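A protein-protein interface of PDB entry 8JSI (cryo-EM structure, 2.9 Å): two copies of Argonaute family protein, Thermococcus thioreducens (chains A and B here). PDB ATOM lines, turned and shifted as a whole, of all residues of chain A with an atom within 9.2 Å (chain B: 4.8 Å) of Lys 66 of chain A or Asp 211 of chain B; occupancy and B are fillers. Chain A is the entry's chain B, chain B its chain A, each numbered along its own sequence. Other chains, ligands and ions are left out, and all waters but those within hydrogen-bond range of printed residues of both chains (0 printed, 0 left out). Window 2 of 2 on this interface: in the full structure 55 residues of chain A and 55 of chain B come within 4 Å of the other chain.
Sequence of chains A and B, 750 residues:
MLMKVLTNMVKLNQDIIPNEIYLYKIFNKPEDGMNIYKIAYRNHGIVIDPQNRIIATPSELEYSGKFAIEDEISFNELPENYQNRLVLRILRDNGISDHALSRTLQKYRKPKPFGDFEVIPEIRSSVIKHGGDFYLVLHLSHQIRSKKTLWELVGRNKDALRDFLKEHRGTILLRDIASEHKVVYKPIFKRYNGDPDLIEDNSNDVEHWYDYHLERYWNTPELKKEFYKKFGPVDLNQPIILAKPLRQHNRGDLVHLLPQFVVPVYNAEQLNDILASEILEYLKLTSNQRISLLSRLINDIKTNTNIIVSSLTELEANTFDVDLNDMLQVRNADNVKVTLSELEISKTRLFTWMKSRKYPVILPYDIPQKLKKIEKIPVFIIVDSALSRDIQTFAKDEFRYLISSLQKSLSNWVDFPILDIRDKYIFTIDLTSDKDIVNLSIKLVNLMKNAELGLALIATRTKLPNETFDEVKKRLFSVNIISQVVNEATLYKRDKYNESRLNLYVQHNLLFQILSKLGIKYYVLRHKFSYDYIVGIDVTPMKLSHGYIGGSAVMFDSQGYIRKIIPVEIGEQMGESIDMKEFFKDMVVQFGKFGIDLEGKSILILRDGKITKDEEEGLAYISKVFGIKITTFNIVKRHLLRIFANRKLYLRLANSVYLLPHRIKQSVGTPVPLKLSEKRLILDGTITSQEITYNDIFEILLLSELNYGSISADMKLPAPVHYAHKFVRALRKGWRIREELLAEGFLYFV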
ATOM      1  N   TYR A  24      -0.719 -19.910  -3.634  1.00  0.00           N
ATOM      2  CA  TYR A  24       0.586 -20.508  -3.866  1.00  0.00           C
ATOM      3  C   TYR A  24       0.732 -21.764  -3.021  1.00  0.00           C
ATOM      4  O   TYR A  24       0.214 -21.845  -1.905  1.00  0.00           O
ATOM      5  CB  TYR A  24       1.709 -19.520  -3.536  1.00  0.00           C
ATOM      6  CG  TYR A  24       1.891 -18.446  -4.580  1.00  0.00           C
ATOM      7  CD1 TYR A  24       1.583 -18.687  -5.909  1.00  0.00           C
ATOM      8  CD2 TYR A  24       2.347 -17.184  -4.234  1.00  0.00           C
ATOM      9  CE1 TYR A  24       1.740 -17.708  -6.866  1.00  0.00           C
ATOM     10  CE2 TYR A  24       2.504 -16.197  -5.185  1.00  0.00           C
ATOM     11  CZ  TYR A  24       2.202 -16.464  -6.499  1.00  0.00           C
ATOM     12  OH  TYR A  24       2.360 -15.485  -7.451  1.00  0.00           O
ATOM     13  N   LYS A  25       1.441 -22.747  -3.567  1.00  0.00           N
ATOM     14  CA  LYS A  25       1.711 -23.999  -2.875  1.00  0.00           C
ATOM     15  C   LYS A  25       3.200 -24.103  -2.576  1.00  0.00           C
ATOM     16  O   LYS A  25       4.034 -23.959  -3.474  1.00  0.00           O
ATOM     17  CB  LYS A  25       1.260 -25.204  -3.702  1.00  0.00           C
ATOM     18  CG  LYS A  25       1.473 -26.537  -3.009  1.00  0.00           C
ATOM     19  CD  LYS A  25       0.866 -27.678  -3.802  1.00  0.00           C
ATOM     20  CE  LYS A  25      -0.179 -28.417  -2.986  1.00  0.00           C
ATOM     21  NZ  LYS A  25      -1.349 -28.810  -3.817  1.00  0.00           N
ATOM     22  N   ILE A  26       3.526 -24.359  -1.313  1.00  0.00           N
ATOM     23  CA  ILE A  26       4.905 -24.444  -0.848  1.00  0.00           C
ATOM     24  C   ILE A  26       5.278 -25.915  -0.738  1.00  0.00           C
ATOM     25  O   ILE A  26       4.598 -26.685  -0.050  1.00  0.00           O
ATOM     26  CB  ILE A  26       5.095 -23.727   0.496  1.00  0.00           C
ATOM     27  CG1 ILE A  26       4.602 -22.281   0.402  1.00  0.00           C
ATOM     28  CG2 ILE A  26       6.549 -23.787   0.931  1.00  0.00           C
ATOM     29  CD1 ILE A  26       5.601 -21.330  -0.217  1.00  0.00           C
ATOM     30  N   PHE A  27       6.353 -26.307  -1.417  1.00  0.00           N
ATOM     31  CA  PHE A  27       6.869 -27.672  -1.347  1.00  0.00           C
ATOM     32  C   PHE A  27       8.033 -27.684  -0.366  1.00  0.00           C
ATOM     33  O   PHE A  27       9.144 -27.258  -0.693  1.00  0.00           O
ATOM     34  CB  PHE A  27       7.291 -28.170  -2.725  1.00  0.00           C
ATOM     35  CG  PHE A  27       6.146 -28.376  -3.669  1.00  0.00           C
ATOM     36  CD1 PHE A  27       5.483 -29.587  -3.718  1.00  0.00           C
ATOM     37  CD2 PHE A  27       5.724 -27.355  -4.501  1.00  0.00           C
ATOM     38  CE1 PHE A  27       4.426 -29.779  -4.581  1.00  0.00           C
ATOM     39  CE2 PHE A  27       4.667 -27.541  -5.367  1.00  0.00           C
ATOM     40  CZ  PHE A  27       4.017 -28.754  -5.406  1.00  0.00           C
ATOM     41  N   ASN A  28       7.775 -28.170   0.844  1.00  0.00           N
ATOM     42  CA  ASN A  28       8.790 -28.190   1.890  1.00  0.00           C
ATOM     43  C   ASN A  28       8.393 -29.227   2.929  1.00  0.00           C
ATOM     44  O   ASN A  28       7.228 -29.623   3.013  1.00  0.00           O
ATOM     45  CB  ASN A  28       8.951 -26.809   2.527  1.00  0.00           C
ATOM     46  CG  ASN A  28      10.257 -26.663   3.271  1.00  0.00           C
ATOM     47  OD1 ASN A  28      10.820 -27.643   3.755  1.00  0.00           O
ATOM     48  ND2 ASN A  28      10.751 -25.435   3.366  1.00  0.00           N
ATOM     49  N   LYS A  29       9.371 -29.664   3.718  1.00  0.00           N
ATOM     50  CA  LYS A  29       9.112 -30.642   4.758  1.00  0.00           C
ATOM     51  C   LYS A  29       9.160 -29.977   6.130  1.00  0.00           C
ATOM     52  O   LYS A  29       9.970 -29.074   6.359  1.00  0.00           O
ATOM     53  CB  LYS A  29      10.134 -31.779   4.692  1.00  0.00           C
ATOM     54  CG  LYS A  29       9.547 -33.095   4.212  1.00  0.00           C
ATOM     55  CD  LYS A  29      10.602 -33.964   3.550  1.00  0.00           C
ATOM     56  CE  LYS A  29       9.968 -35.151   2.844  1.00  0.00           C
ATOM     57  NZ  LYS A  29       9.520 -36.195   3.803  1.00  0.00           N
ATOM     58  N   ILE A  39       6.447 -17.867   7.125  1.00  0.00           N
ATOM     59  CA  ILE A  39       6.660 -17.517   5.724  1.00  0.00           C
ATOM     60  C   ILE A  39       5.501 -16.674   5.210  1.00  0.00           C
ATOM     61  O   ILE A  39       5.695 -15.594   4.636  1.00  0.00           O
ATOM     62  CB  ILE A  39       6.842 -18.788   4.876  1.00  0.00           C
ATOM     63  CG1 ILE A  39       8.017 -19.617   5.393  1.00  0.00           C
ATOM     64  CG2 ILE A  39       7.041 -18.429   3.413  1.00  0.00           C
ATOM     65  CD1 ILE A  39       7.951 -21.075   4.996  1.00  0.00           C
ATOM     66  N   ARG A  53      -0.179 -26.954   2.419  1.00  0.00           N
ATOM     67  CA  ARG A  53       0.736 -25.813   2.387  1.00  0.00           C
ATOM     68  C   ARG A  53       0.338 -24.815   1.299  1.00  0.00           C
ATOM     69  O   ARG A  53       1.140 -24.435   0.445  1.00  0.00           O
ATOM     70  CB  ARG A  53       2.186 -26.273   2.211  1.00  0.00           C
ATOM     71  CG  ARG A  53       2.615 -27.358   3.186  1.00  0.00           C
ATOM     72  CD  ARG A  53       3.709 -28.226   2.593  1.00  0.00           C
ATOM     73  NE  ARG A  53       3.444 -28.540   1.193  1.00  0.00           N
ATOM     74  CZ  ARG A  53       2.955 -29.694   0.764  1.00  0.00           C
ATOM     75  NH1 ARG A  53       2.677 -30.681   1.600  1.00  0.00           N
ATOM     76  NH2 ARG A  53       2.736 -29.863  -0.537  1.00  0.00           N
ATOM     77  N   LEU A  61       4.911 -13.982  -4.999  1.00  0.00           N
ATOM     78  CA  LEU A  61       5.765 -14.497  -3.940  1.00  0.00           C
ATOM     79  C   LEU A  61       7.220 -14.089  -4.160  1.00  0.00           C
ATOM     80  O   LEU A  61       7.654 -13.794  -5.276  1.00  0.00           O
ATOM     81  CB  LEU A  61       5.665 -16.020  -3.862  1.00  0.00           C
ATOM     82  CG  LEU A  61       5.827 -16.653  -2.480  1.00  0.00           C
ATOM     83  CD1 LEU A  61       4.921 -15.972  -1.471  1.00  0.00           C
ATOM     84  CD2 LEU A  61       5.541 -18.143  -2.540  1.00  0.00           C
ATOM     85  N   GLU A  62       7.974 -14.077  -3.065  1.00  0.00           N
ATOM     86  CA  GLU A  62       9.406 -13.808  -3.075  1.00  0.00           C
ATOM     87  C   GLU A  62      10.151 -14.885  -2.302  1.00  0.00           C
ATOM     88  O   GLU A  62      11.173 -14.629  -1.660  1.00  0.00           O
ATOM     89  CB  GLU A  62       9.709 -12.425  -2.506  1.00  0.00           C
ATOM     90  CG  GLU A  62      10.699 -11.618  -3.332  1.00  0.00           C
ATOM     91  CD  GLU A  62      10.188 -11.326  -4.729  1.00  0.00           C
ATOM     92  OE1 GLU A  62       8.968 -11.112  -4.882  1.00  0.00           O
ATOM     93  OE2 GLU A  62      11.005 -11.313  -5.674  1.00  0.00           O
ATOM     94  N   TYR A  63       9.639 -16.112  -2.353  1.00  0.00           N
ATOM     95  CA  TYR A  63      10.241 -17.226  -1.641  1.00  0.00           C
ATOM     96  C   TYR A  63      11.547 -17.646  -2.314  1.00  0.00           C
ATOM     97  O   TYR A  63      11.813 -17.332  -3.479  1.00  0.00           O
ATOM     98  CB  TYR A  63       9.268 -18.402  -1.583  1.00  0.00           C
ATOM     99  CG  TYR A  63       9.565 -19.413  -0.500  1.00  0.00           C
ATOM    100  CD1 TYR A  63      10.190 -19.034   0.679  1.00  0.00           C
ATOM    101  CD2 TYR A  63       9.216 -20.746  -0.657  1.00  0.00           C
ATOM    102  CE1 TYR A  63      10.462 -19.957   1.669  1.00  0.00           C
ATOM    103  CE2 TYR A  63       9.482 -21.674   0.326  1.00  0.00           C
ATOM    104  CZ  TYR A  63      10.104 -21.276   1.487  1.00  0.00           C
ATOM    105  OH  TYR A  63      10.371 -22.202   2.469  1.00  0.00           O
ATOM    106  N   SER A  64      12.373 -18.367  -1.558  1.00  0.00           N
ATOM    107  CA  SER A  64      13.640 -18.888  -2.056  1.00  0.00           C
ATOM    108  C   SER A  64      13.570 -20.362  -2.429  1.00  0.00           C
ATOM    109  O   SER A  64      14.290 -20.801  -3.329  1.00  0.00           O
ATOM    110  CB  SER A  64      14.744 -18.680  -1.015  1.00  0.00           C
ATOM    111  OG  SER A  64      14.848 -17.316  -0.648  1.00  0.00           O
ATOM    112  N   GLY A  65      12.720 -21.135  -1.760  1.00  0.00           N
ATOM    113  CA  GLY A  65      12.611 -22.554  -2.033  1.00  0.00           C
ATOM    114  C   GLY A  65      11.751 -22.875  -3.236  1.00  0.00           C
ATOM    115  O   GLY A  65      11.761 -22.143  -4.230  1.00  0.00           O
ATOM    116  N   LYS A  66      11.000 -23.970  -3.158  1.00  0.00           N
ATOM    117  CA  LYS A  66      10.148 -24.407  -4.254  1.00  0.00           C
ATOM    118  C   LYS A  66       8.707 -23.993  -3.991  1.00  0.00           C
ATOM    119  O   LYS A  66       8.176 -24.229  -2.901  1.00  0.00           O
ATOM    120  CB  LYS A  66      10.234 -25.923  -4.433  1.00  0.00           C
ATOM    121  CG  LYS A  66      11.469 -26.396  -5.179  1.00  0.00           C
ATOM    122  CD  LYS A  66      11.129 -27.523  -6.140  1.00  0.00           C
ATOM    123  CE  LYS A  66      12.170 -27.642  -7.240  1.00  0.00           C
ATOM    124  NZ  LYS A  66      11.550 -27.635  -8.593  1.00  0.00           N
ATOM    125  N   PHE A  67       8.079 -23.376  -4.990  1.00  0.00           N
ATOM    126  CA  PHE A  67       6.671 -23.018  -4.923  1.00  0.00           C
ATOM    127  C   PHE A  67       6.047 -23.249  -6.293  1.00  0.00           C
ATOM    128  O   PHE A  67       6.743 -23.484  -7.284  1.00  0.00           O
ATOM    129  CB  PHE A  67       6.479 -21.571  -4.450  1.00  0.00           C
ATOM    130  CG  PHE A  67       7.198 -20.553  -5.288  1.00  0.00           C
ATOM    131  CD1 PHE A  67       6.589 -19.995  -6.401  1.00  0.00           C
ATOM    132  CD2 PHE A  67       8.478 -20.142  -4.956  1.00  0.00           C
ATOM    133  CE1 PHE A  67       7.246 -19.056  -7.170  1.00  0.00           C
ATOM    134  CE2 PHE A  67       9.138 -19.203  -5.721  1.00  0.00           C
ATOM    135  CZ  PHE A  67       8.521 -18.660  -6.829  1.00  0.00           C
ATOM    136  N   ALA A  68       4.718 -23.184  -6.345  1.00  0.00           N
ATOM    137  CA  ALA A  68       4.000 -23.410  -7.592  1.00  0.00           C
ATOM    138  C   ALA A  68       2.726 -22.581  -7.587  1.00  0.00           C
ATOM    139  O   ALA A  68       2.016 -22.541  -6.578  1.00  0.00           O
ATOM    140  CB  ALA A  68       3.672 -24.894  -7.779  1.00  0.00           C
ATOM    141  N   ILE A  69       2.442 -21.926  -8.714  1.00  0.00           N
ATOM    142  CA  ILE A  69       1.225 -21.135  -8.826  1.00  0.00           C
ATOM    143  C   ILE A  69       0.023 -22.067  -8.870  1.00  0.00           C
ATOM    144  O   ILE A  69       0.001 -23.052  -9.620  1.00  0.00           O
ATOM    145  CB  ILE A  69       1.274 -20.231 -10.071  1.00  0.00           C
ATOM    146  CG1 ILE A  69       2.410 -19.210  -9.963  1.00  0.00           C
ATOM    147  CG2 ILE A  69      -0.055 -19.521 -10.269  1.00  0.00           C
ATOM    148  CD1 ILE A  69       3.726 -19.669 -10.558  1.00  0.00           C
ATOM    149  N   GLU B 207       6.327 -34.675  -9.569  1.00  0.00           N
ATOM    150  CA  GLU B 207       7.544 -34.111 -10.141  1.00  0.00           C
ATOM    151  C   GLU B 207       8.167 -33.072  -9.220  1.00  0.00           C
ATOM    152  O   GLU B 207       9.395 -33.030  -9.074  1.00  0.00           O
ATOM    153  CB  GLU B 207       7.243 -33.496 -11.506  1.00  0.00           C
ATOM    154  CG  GLU B 207       8.452 -32.893 -12.196  1.00  0.00           C
ATOM    155  CD  GLU B 207       8.585 -33.345 -13.636  1.00  0.00           C
ATOM    156  OE1 GLU B 207       7.628 -33.952 -14.161  1.00  0.00           O
ATOM    157  OE2 GLU B 207       9.647 -33.094 -14.242  1.00  0.00           O
ATOM    158  N   HIS B 208       7.342 -32.231  -8.590  1.00  0.00           N
ATOM    159  CA  HIS B 208       7.877 -31.206  -7.701  1.00  0.00           C
ATOM    160  C   HIS B 208       8.568 -31.819  -6.488  1.00  0.00           C
ATOM    161  O   HIS B 208       9.650 -31.368  -6.101  1.00  0.00           O
ATOM    162  CB  HIS B 208       6.762 -30.257  -7.270  1.00  0.00           C
ATOM    163  CG  HIS B 208       6.459 -29.192  -8.278  1.00  0.00           C
ATOM    164  ND1 HIS B 208       5.357 -29.240  -9.103  1.00  0.00           N
ATOM    165  CD2 HIS B 208       7.121 -28.056  -8.599  1.00  0.00           C
ATOM    166  CE1 HIS B 208       5.349 -28.178  -9.886  1.00  0.00           C
ATOM    167  NE2 HIS B 208       6.408 -27.442  -9.600  1.00  0.00           N
ATOM    168  N   TRP B 209       7.970 -32.849  -5.884  1.00  0.00           N
ATOM    169  CA  TRP B 209       8.612 -33.524  -4.759  1.00  0.00           C
ATOM    170  C   TRP B 209       9.900 -34.214  -5.188  1.00  0.00           C
ATOM    171  O   TRP B 209      10.903 -34.176  -4.463  1.00  0.00           O
ATOM    172  CB  TRP B 209       7.652 -34.533  -4.131  1.00  0.00           C
ATOM    173  CG  TRP B 209       6.632 -33.929  -3.213  1.00  0.00           C
ATOM    174  CD1 TRP B 209       5.276 -34.009  -3.331  1.00  0.00           C
ATOM    175  CD2 TRP B 209       6.887 -33.164  -2.028  1.00  0.00           C
ATOM    176  NE1 TRP B 209       4.671 -33.337  -2.300  1.00  0.00           N
ATOM    177  CE2 TRP B 209       5.637 -32.810  -1.485  1.00  0.00           C
ATOM    178  CE3 TRP B 209       8.048 -32.744  -1.377  1.00  0.00           C
ATOM    179  CZ2 TRP B 209       5.518 -32.055  -0.322  1.00  0.00           C
ATOM    180  CZ3 TRP B 209       7.926 -31.994  -0.223  1.00  0.00           C
ATOM    181  CH2 TRP B 209       6.671 -31.657   0.293  1.00  0.00           C
ATOM    182  N   TYR B 210       9.891 -34.856  -6.360  1.00  0.00           N
ATOM    183  CA  TYR B 210      11.098 -35.515  -6.848  1.00  0.00           C
ATOM    184  C   TYR B 210      12.234 -34.516  -7.020  1.00  0.00           C
ATOM    185  O   TYR B 210      13.351 -34.736  -6.539  1.00  0.00           O
ATOM    186  CB  TYR B 210      10.806 -36.238  -8.162  1.00  0.00           C
ATOM    187  CG  TYR B 210      11.957 -37.074  -8.675  1.00  0.00           C
ATOM    188  CD1 TYR B 210      12.918 -36.529  -9.514  1.00  0.00           C
ATOM    189  CD2 TYR B 210      12.081 -38.407  -8.317  1.00  0.00           C
ATOM    190  CE1 TYR B 210      13.969 -37.289  -9.982  1.00  0.00           C
ATOM    191  CE2 TYR B 210      13.129 -39.175  -8.781  1.00  0.00           C
ATOM    192  CZ  TYR B 210      14.070 -38.612  -9.612  1.00  0.00           C
ATOM    193  OH  TYR B 210      15.116 -39.376 -10.075  1.00  0.00           O
ATOM    194  N   ASP B 211      11.962 -33.396  -7.696  1.00  0.00           N
ATOM    195  CA  ASP B 211      12.995 -32.384  -7.878  1.00  0.00           C
ATOM    196  C   ASP B 211      13.410 -31.731  -6.566  1.00  0.00           C
ATOM    197  O   ASP B 211      14.587 -31.392  -6.407  1.00  0.00           O
ATOM    198  CB  ASP B 211      12.531 -31.318  -8.871  1.00  0.00           C
ATOM    199  CG  ASP B 211      12.391 -31.857 -10.279  1.00  0.00           C
ATOM    200  OD1 ASP B 211      13.429 -32.117 -10.922  1.00  0.00           O
ATOM    201  OD2 ASP B 211      11.247 -32.012 -10.753  1.00  0.00           O
ATOM    202  N   TYR B 212      12.479 -31.551  -5.626  1.00  0.00           N
ATOM    203  CA  TYR B 212      12.837 -30.993  -4.328  1.00  0.00           C
ATOM    204  C   TYR B 212      13.810 -31.903  -3.593  1.00  0.00           C
ATOM    205  O   TYR B 212      14.806 -31.436  -3.030  1.00  0.00           O
ATOM    206  CB  TYR B 212      11.581 -30.764  -3.488  1.00  0.00           C
ATOM    207  CG  TYR B 212      11.870 -30.476  -2.034  1.00  0.00           C
ATOM    208  CD1 TYR B 212      12.576 -29.342  -1.657  1.00  0.00           C
ATOM    209  CD2 TYR B 212      11.446 -31.343  -1.038  1.00  0.00           C
ATOM    210  CE1 TYR B 212      12.847 -29.078  -0.330  1.00  0.00           C
ATOM    211  CE2 TYR B 212      11.711 -31.088   0.291  1.00  0.00           C
ATOM    212  CZ  TYR B 212      12.411 -29.955   0.640  1.00  0.00           C
ATOM    213  OH  TYR B 212      12.677 -29.696   1.963  1.00  0.00           O
ATOM    214  N   HIS B 213      13.541 -33.210  -3.590  1.00  0.00           N
ATOM    215  CA  HIS B 213      14.462 -34.138  -2.942  1.00  0.00           C
ATOM    216  C   HIS B 213      15.785 -34.222  -3.690  1.00  0.00           C
ATOM    217  O   HIS B 213      16.841 -34.410  -3.074  1.00  0.00           O
ATOM    218  CB  HIS B 213      13.831 -35.522  -2.821  1.00  0.00           C
ATOM    219  CG  HIS B 213      12.845 -35.641  -1.702  1.00  0.00           C
ATOM    220  ND1 HIS B 213      11.514 -35.317  -1.843  1.00  0.00           N
ATOM    221  CD2 HIS B 213      13.000 -36.047  -0.420  1.00  0.00           C
ATOM    222  CE1 HIS B 213      10.890 -35.519  -0.697  1.00  0.00           C
ATOM    223  NE2 HIS B 213      11.769 -35.963   0.183  1.00  0.00           N
ATOM    224  N   LEU B 214      15.754 -34.088  -5.018  1.00  0.00           N
ATOM    225  CA  LEU B 214      16.986 -34.199  -5.791  1.00  0.00           C
ATOM    226  C   LEU B 214      17.906 -33.009  -5.553  1.00  0.00           C
ATOM    227  O   LEU B 214      19.099 -33.184  -5.289  1.00  0.00           O
ATOM    228  CB  LEU B 214      16.663 -34.337  -7.278  1.00  0.00           C
ATOM    229  CG  LEU B 214      17.846 -34.224  -8.241  1.00  0.00           C
ATOM    230  CD1 LEU B 214      18.874 -35.309  -7.966  1.00  0.00           C
ATOM    231  CD2 LEU B 214      17.370 -34.289  -9.681  1.00  0.00           C
ATOM    232  N   GLU B 215      17.374 -31.788  -5.634  1.00  0.00           N
ATOM    233  CA  GLU B 215      18.198 -30.587  -5.590  1.00  0.00           C
ATOM    234  C   GLU B 215      18.334 -30.002  -4.189  1.00  0.00           C
ATOM    235  O   GLU B 215      18.634 -28.813  -4.053  1.00  0.00           O
ATOM    236  CB  GLU B 215      17.641 -29.528  -6.544  1.00  0.00           C
ATOM    237  CG  GLU B 215      17.078 -30.084  -7.840  1.00  0.00           C
ATOM    238  CD  GLU B 215      16.147 -29.110  -8.537  1.00  0.00           C
ATOM    239  OE1 GLU B 215      16.224 -27.899  -8.242  1.00  0.00           O
ATOM    240  OE2 GLU B 215      15.338 -29.555  -9.378  1.00  0.00           O
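OD2 of Asp 211 of chain B sits close to O of Glu 207 of chain B (2.7 Å). The backbone carbonyl oxygen (O) of Trp 209 of chain B sits at hydrogen-bond distance from a ring nitrogen (ND1) of His 213 of chain B (2.9 Å). The backbone carbonyl oxygen (O) of Ile 26 of chain A sits at hydrogen-bond distance from the guanidinium group (NE) of Arg 53 of chain A (2.5 Å). N of Phe 27 of chain A lies within hydrogen-bond range of O of Lys 66 of chain A, 3.1 Å away. ND2 of Asn 28 of chain A lies within hydrogen-bond range of OH of Tyr 63 of chain A, at 3.4 Å.
No position is printed for both chains. Of the 8 pairs that touch across the chains among the printed residues, none has its exchanged pair printed and touching as well.
The side-chain hydroxyl (OH) of Tyr 212 of chain B lies within hydrogen-bond range of the side-chain amide oxygen (OD1) of Asn 28 of chain A (3.3 Å).
Lys 66 of chain A touches just one residue of chain B: Asp 211. Of the printed residues of chain A, Asp 211 of chain B touches Lys 66. Of the printed residues of chain A, His 213 of chain B touches Lys 29. Printed residues of chain B within 4 Å of Arg 53 of chain A: Trp 209. Printed residues of chain A within 4 Å of Tyr 212 of chain B: Asn 28 (3.3 Å) and Lys 29 (3.7 Å). Of the printed residues of chain B, Asn 28 of chain A touches Trp 209 and Tyr 212. Tyr 210 of chain B touches none of the printed residues of chain A. Tyr 63 of chain A touches none of the printed residues of chain B. The nearest residue of chain B that does not touch Lys 66 of chain A is His 208 of chain B (4.1 Å).
Among the printed residues, merely in contact across the chains: Phe 27 of chain A with His 208 of chain B, Phe 27 of chain A with Trp 209 of chain B, Asn 28 of chain A with Trp 209 of chain B, Lys 29 of chain A with Tyr 212 of chain B, Lys 29 of chain A with His 213 of chain B, Arg 53 of chain A with Trp 209 of chain B and Lys 66 of chain A with Asp 211 of chain B.
Of the 9 printed residues of chain B, 5 touch a printed residue of chain A. Hydrophobic or aromatic side chains of chain B within 4 Å of the printed part of chain A: His 208, Trp 209, Tyr 212 and His 213. Of the 17 printed residues of chain A, 5 touch a printed residue of chain B. Printed residues of chain A that touch a printed residue of chain B: Phe 27, Asn 28, Lys 29, Arg 53 and Lys 66. Hydrophobic or aromatic side chains of chain A that line the printed part of chain B: Phe 27. Among the printed residues, 8 pairs touch across the chains.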
